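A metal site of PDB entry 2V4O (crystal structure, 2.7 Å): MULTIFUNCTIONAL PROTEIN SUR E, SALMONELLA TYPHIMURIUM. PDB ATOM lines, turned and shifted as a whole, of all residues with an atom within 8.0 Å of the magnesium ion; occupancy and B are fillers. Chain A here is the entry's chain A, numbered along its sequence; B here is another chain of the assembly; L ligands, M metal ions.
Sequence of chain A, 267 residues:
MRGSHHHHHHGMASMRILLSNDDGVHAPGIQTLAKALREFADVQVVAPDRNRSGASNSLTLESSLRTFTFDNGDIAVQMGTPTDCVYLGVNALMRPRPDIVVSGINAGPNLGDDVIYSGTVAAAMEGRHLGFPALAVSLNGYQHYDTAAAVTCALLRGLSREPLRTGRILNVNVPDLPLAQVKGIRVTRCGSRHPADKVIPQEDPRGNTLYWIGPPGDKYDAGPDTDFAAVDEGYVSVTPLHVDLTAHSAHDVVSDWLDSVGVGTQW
Within 4 Å of the magnesium ion: Asp 22, Asp 23, Ser 53 and Asn 106. The nearest printed residue that does not touch the magnesium ion is Thr 120 (4.6 Å).
The magnesium ion is bound by the side-chain carboxylate of Asp 23, an oxygen (O3) of the ligand, the side-chain amide nitrogen of Asn 106, the side-chain carboxylate of Asp 22 and the side-chain hydroxyl of Ser 53. The magnesium ion has five donor atoms within binding distance.
The backbone NH of Ala 107 sits at hydrogen-bond distance from the side-chain carboxylate of Asp 23 (3.1 Å). The side-chain amide oxygen (OD1) of Asn 106 lies within hydrogen-bond range of the side-chain amide nitrogen (ND2) of Asn 110. N of Ser 53 sits close to ND2 of Asn 51 (3.0 Å). OD1 of Asp 22 lies within hydrogen-bond range of N of Gly 119 (3.3 Å). The side-chain amide oxygen (OD1) of Asn 21 sits at hydrogen-bond distance from the backbone NH (N) of Asp 23, 3.2 Å away. N of Arg 52 sits at hydrogen-bond distance from O of Asp 22 (2.8 Å). The side-chain amide nitrogen (ND2) of Asn 106 lies close to the side-chain hydroxyl (OG1) of Thr 120 (3.0 Å). The side-chain amide oxygen of Asn 106 lies close to the backbone carbonyl oxygen of Gly 108 (3.0 Å).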
ATOM      1  N   ASN A  21      28.412  25.555  25.520  1.00  0.00           N
ATOM      2  CA  ASN A  21      28.386  24.157  25.974  1.00  0.00           C
ATOM      3  C   ASN A  21      27.211  23.537  25.214  1.00  0.00           C
ATOM      4  O   ASN A  21      26.618  24.216  24.375  1.00  0.00           O
ATOM      5  CB  ASN A  21      28.170  24.060  27.493  1.00  0.00           C
ATOM      6  CG  ASN A  21      26.698  24.126  27.926  1.00  0.00           C
ATOM      7  OD1 ASN A  21      25.806  24.435  27.151  1.00  0.00           O
ATOM      8  ND2 ASN A  21      26.475  23.857  29.182  1.00  0.00           N
ATOM      9  N   ASP A  22      26.844  22.289  25.511  1.00  0.00           N
ATOM     10  CA  ASP A  22      25.573  21.796  24.962  1.00  0.00           C
ATOM     11  C   ASP A  22      24.526  21.404  26.000  1.00  0.00           C
ATOM     12  O   ASP A  22      23.396  21.097  25.615  1.00  0.00           O
ATOM     13  CB  ASP A  22      25.750  20.691  23.921  1.00  0.00           C
ATOM     14  CG  ASP A  22      26.044  19.329  24.519  1.00  0.00           C
ATOM     15  OD1 ASP A  22      26.316  18.421  23.723  1.00  0.00           O
ATOM     16  OD2 ASP A  22      26.029  19.135  25.759  1.00  0.00           O
ATOM     17  N   ASP A  23      24.864  21.402  27.285  1.00  0.00           N
ATOM     18  CA  ASP A  23      23.883  21.010  28.304  1.00  0.00           C
ATOM     19  C   ASP A  23      22.936  22.146  28.664  1.00  0.00           C
ATOM     20  O   ASP A  23      21.928  21.901  29.330  1.00  0.00           O
ATOM     21  CB  ASP A  23      24.549  20.444  29.556  1.00  0.00           C
ATOM     22  CG  ASP A  23      25.407  19.265  29.229  1.00  0.00           C
ATOM     23  OD1 ASP A  23      24.936  18.410  28.444  1.00  0.00           O
ATOM     24  OD2 ASP A  23      26.561  19.199  29.737  1.00  0.00           O
ATOM     25  N   GLY A  24      23.270  23.357  28.225  1.00  0.00           N
ATOM     26  CA  GLY A  24      22.450  24.517  28.422  1.00  0.00           C
ATOM     27  C   GLY A  24      23.198  25.517  29.289  1.00  0.00           C
ATOM     28  O   GLY A  24      24.097  25.147  30.089  1.00  0.00           O
ATOM     29  N   ALA A  27      23.654  24.856  33.095  1.00  0.00           N
ATOM     30  CA  ALA A  27      24.235  23.627  33.591  1.00  0.00           C
ATOM     31  C   ALA A  27      25.414  23.858  34.572  1.00  0.00           C
ATOM     32  O   ALA A  27      26.192  24.829  34.450  1.00  0.00           O
ATOM     33  CB  ALA A  27      24.653  22.800  32.420  1.00  0.00           C
ATOM     34  N   ASN A  51      18.785  21.610  27.642  1.00  0.00           N
ATOM     35  CA  ASN A  51      19.793  20.596  27.498  1.00  0.00           C
ATOM     36  C   ASN A  51      19.675  20.074  26.126  1.00  0.00           C
ATOM     37  O   ASN A  51      18.647  19.524  25.758  1.00  0.00           O
ATOM     38  CB  ASN A  51      19.578  19.456  28.450  1.00  0.00           C
ATOM     39  CG  ASN A  51      20.690  18.439  28.370  1.00  0.00           C
ATOM     40  OD1 ASN A  51      21.401  18.227  29.338  1.00  0.00           O
ATOM     41  ND2 ASN A  51      20.884  17.858  27.217  1.00  0.00           N
ATOM     42  N   ARG A  52      20.741  20.164  25.377  1.00  0.00           N
ATOM     43  CA  ARG A  52      20.651  19.909  23.960  1.00  0.00           C
ATOM     44  C   ARG A  52      21.623  18.807  23.529  1.00  0.00           C
ATOM     45  O   ARG A  52      22.182  18.820  22.432  1.00  0.00           O
ATOM     46  CB  ARG A  52      20.942  21.214  23.259  1.00  0.00           C
ATOM     47  CG  ARG A  52      20.180  21.402  22.094  1.00  0.00           C
ATOM     48  CD  ARG A  52      18.765  21.620  22.410  1.00  0.00           C
ATOM     49  NE  ARG A  52      18.210  22.459  21.335  1.00  0.00           N
ATOM     50  CZ  ARG A  52      17.917  22.017  20.119  1.00  0.00           C
ATOM     51  NH1 ARG A  52      18.107  20.735  19.834  1.00  0.00           N
ATOM     52  NH2 ARG A  52      17.427  22.850  19.216  1.00  0.00           N
ATOM     53  N   SER A  53      21.809  17.842  24.409  1.00  0.00           N
ATOM     54  CA  SER A  53      22.822  16.817  24.235  1.00  0.00           C
ATOM     55  C   SER A  53      22.298  15.979  23.114  1.00  0.00           C
ATOM     56  O   SER A  53      21.093  15.828  22.988  1.00  0.00           O
ATOM     57  CB  SER A  53      23.002  15.992  25.504  1.00  0.00           C
ATOM     58  OG  SER A  53      23.093  16.858  26.603  1.00  0.00           O
ATOM     59  N   GLY A  54      23.232  15.449  22.316  1.00  0.00           N
ATOM     60  CA  GLY A  54      22.902  14.707  21.102  1.00  0.00           C
ATOM     61  C   GLY A  54      22.766  15.581  19.861  1.00  0.00           C
ATOM     62  O   GLY A  54      22.472  15.057  18.790  1.00  0.00           O
ATOM     63  N   ALA A  55      22.953  16.893  19.983  1.00  0.00           N
ATOM     64  CA  ALA A  55      22.599  17.797  18.884  1.00  0.00           C
ATOM     65  C   ALA A  55      23.544  17.732  17.674  1.00  0.00           C
ATOM     66  O   ALA A  55      23.195  18.223  16.577  1.00  0.00           O
ATOM     67  CB  ALA A  55      22.455  19.210  19.356  1.00  0.00           C
ATOM     68  N   GLY A 104      31.725  24.255  26.981  1.00  0.00           N
ATOM     69  CA  GLY A 104      31.612  24.268  28.499  1.00  0.00           C
ATOM     70  C   GLY A 104      31.734  22.892  29.051  1.00  0.00           C
ATOM     71  O   GLY A 104      31.644  21.957  28.261  1.00  0.00           O
ATOM     72  N   ILE A 105      31.967  22.738  30.356  1.00  0.00           N
ATOM     73  CA  ILE A 105      32.302  21.374  30.824  1.00  0.00           C
ATOM     74  C   ILE A 105      31.098  20.437  30.655  1.00  0.00           C
ATOM     75  O   ILE A 105      30.093  20.610  31.305  1.00  0.00           O
ATOM     76  CB  ILE A 105      32.783  21.316  32.267  1.00  0.00           C
ATOM     77  CG1 ILE A 105      33.992  22.244  32.472  1.00  0.00           C
ATOM     78  CG2 ILE A 105      33.192  19.896  32.580  1.00  0.00           C
ATOM     79  N   ASN A 106      31.178  19.481  29.739  1.00  0.00           N
ATOM     80  CA  ASN A 106      30.044  18.600  29.469  1.00  0.00           C
ATOM     81  C   ASN A 106      29.893  17.493  30.483  1.00  0.00           C
ATOM     82  O   ASN A 106      30.852  16.812  30.796  1.00  0.00           O
ATOM     83  CB  ASN A 106      30.175  17.968  28.098  1.00  0.00           C
ATOM     84  CG  ASN A 106      28.947  17.161  27.723  1.00  0.00           C
ATOM     85  OD1 ASN A 106      28.975  15.944  27.756  1.00  0.00           O
ATOM     86  ND2 ASN A 106      27.871  17.852  27.374  1.00  0.00           N
ATOM     87  N   ALA A 107      28.670  17.289  30.951  1.00  0.00           N
ATOM     88  CA  ALA A 107      28.375  16.177  31.867  1.00  0.00           C
ATOM     89  C   ALA A 107      28.387  14.833  31.108  1.00  0.00           C
ATOM     90  O   ALA A 107      27.452  14.530  30.413  1.00  0.00           O
ATOM     91  CB  ALA A 107      27.032  16.411  32.527  1.00  0.00           C
ATOM     92  N   GLY A 108      29.449  14.035  31.233  1.00  0.00           N
ATOM     93  CA  GLY A 108      29.555  12.798  30.473  1.00  0.00           C
ATOM     94  C   GLY A 108      30.627  12.898  29.413  1.00  0.00           C
ATOM     95  O   GLY A 108      30.899  13.977  28.901  1.00  0.00           O
ATOM     96  N   PRO A 109      31.244  11.758  29.052  1.00  0.00           N
ATOM     97  CA  PRO A 109      32.343  11.809  28.094  1.00  0.00           C
ATOM     98  C   PRO A 109      31.923  11.950  26.644  1.00  0.00           C
ATOM     99  O   PRO A 109      30.826  11.571  26.260  1.00  0.00           O
ATOM    100  CB  PRO A 109      33.017  10.428  28.279  1.00  0.00           C
ATOM    101  CG  PRO A 109      31.880   9.535  28.667  1.00  0.00           C
ATOM    102  CD  PRO A 109      30.967  10.377  29.500  1.00  0.00           C
ATOM    103  N   ASN A 110      32.818  12.449  25.840  1.00  0.00           N
ATOM    104  CA  ASN A 110      32.688  12.372  24.412  1.00  0.00           C
ATOM    105  C   ASN A 110      33.960  11.711  23.899  1.00  0.00           C
ATOM    106  O   ASN A 110      34.974  12.380  23.649  1.00  0.00           O
ATOM    107  CB  ASN A 110      32.506  13.758  23.857  1.00  0.00           C
ATOM    108  CG  ASN A 110      31.116  14.270  24.065  1.00  0.00           C
ATOM    109  OD1 ASN A 110      30.181  13.783  23.425  1.00  0.00           O
ATOM    110  ND2 ASN A 110      30.949  15.224  24.992  1.00  0.00           N
ATOM    111  N   SER A 118      28.369  14.544  19.174  1.00  0.00           N
ATOM    112  CA  SER A 118      28.490  15.444  20.308  1.00  0.00           C
ATOM    113  C   SER A 118      28.223  16.910  19.954  1.00  0.00           C
ATOM    114  O   SER A 118      28.861  17.454  19.054  1.00  0.00           O
ATOM    115  CB  SER A 118      29.888  15.313  20.912  1.00  0.00           C
ATOM    116  OG  SER A 118      30.143  16.336  21.860  1.00  0.00           O
ATOM    117  N   GLY A 119      27.312  17.550  20.685  1.00  0.00           N
ATOM    118  CA  GLY A 119      27.051  18.972  20.527  1.00  0.00           C
ATOM    119  C   GLY A 119      28.159  19.816  21.123  1.00  0.00           C
ATOM    120  O   GLY A 119      28.541  20.870  20.575  1.00  0.00           O
ATOM    121  N   THR A 120      28.684  19.356  22.268  1.00  0.00           N
ATOM    122  CA  THR A 120      29.891  19.917  22.874  1.00  0.00           C
ATOM    123  C   THR A 120      31.013  20.102  21.829  1.00  0.00           C
ATOM    124  O   THR A 120      31.556  21.222  21.707  1.00  0.00           O
ATOM    125  CB  THR A 120      30.374  19.005  24.050  1.00  0.00           C
ATOM    126  OG1 THR A 120      29.303  18.844  24.987  1.00  0.00           O
ATOM    127  CG2 THR A 120      31.601  19.583  24.768  1.00  0.00           C
ATOM    128  N   SER A 138      35.078  17.694  28.206  1.00  0.00           N
ATOM    129  CA  SER A 138      34.103  16.726  28.737  1.00  0.00           C
ATOM    130  C   SER A 138      34.567  15.978  30.000  1.00  0.00           C
ATOM    131  O   SER A 138      35.688  15.476  30.078  1.00  0.00           O
ATOM    132  CB  SER A 138      33.754  15.683  27.666  1.00  0.00           C
ATOM    133  OG  SER A 138      33.227  16.286  26.472  1.00  0.00           O
ATOM    134  N   LEU B  61      17.703  12.539  22.131  1.00  0.00           N
ATOM    135  CA  LEU B  61      18.066  11.916  23.406  1.00  0.00           C
ATOM    136  C   LEU B  61      17.157  12.304  24.579  1.00  0.00           C
ATOM    137  O   LEU B  61      16.987  11.515  25.502  1.00  0.00           O
ATOM    138  CB  LEU B  61      19.510  12.256  23.739  1.00  0.00           C
ATOM    139  CG  LEU B  61      20.654  11.270  23.431  1.00  0.00           C
ATOM    140  CD1 LEU B  61      20.471  10.582  22.105  1.00  0.00           C
ATOM    141  CD2 LEU B  61      22.042  11.947  23.514  1.00  0.00           C
ATOM    142  N   GLU B  62      16.598  13.523  24.564  1.00  0.00           N
ATOM    143  CA  GLU B  62      15.746  14.021  25.668  1.00  0.00           C
ATOM    144  C   GLU B  62      14.344  13.455  25.691  1.00  0.00           C
ATOM    145  O   GLU B  62      13.582  13.721  26.600  1.00  0.00           O
ATOM    146  CB  GLU B  62      15.616  15.527  25.619  1.00  0.00           C
ATOM    147  CG  GLU B  62      16.907  16.293  25.995  1.00  0.00           C
ATOM    148  CD  GLU B  62      17.299  16.242  27.522  1.00  0.00           C
ATOM    149  OE1 GLU B  62      16.982  17.243  28.255  1.00  0.00           O
ATOM    150  OE2 GLU B  62      17.932  15.202  27.910  1.00  0.00           O
HETATM  151  P1  LIG L   1      27.088  15.381  24.135  1.00  0.00           P
HETATM  152  O1  LIG L   1      28.387  16.139  24.042  1.00  0.00           O
HETATM  153  O2  LIG L   1      27.238  13.851  24.104  1.00  0.00           O
HETATM  154  O3  LIG L   1      26.469  15.800  25.448  1.00  0.00           O
HETATM  155  O4  LIG L   1      26.143  15.800  23.028  1.00  0.00           O
HETATM  156 MG    MG M   1      25.635  17.030  27.003  1.00  0.00          MG
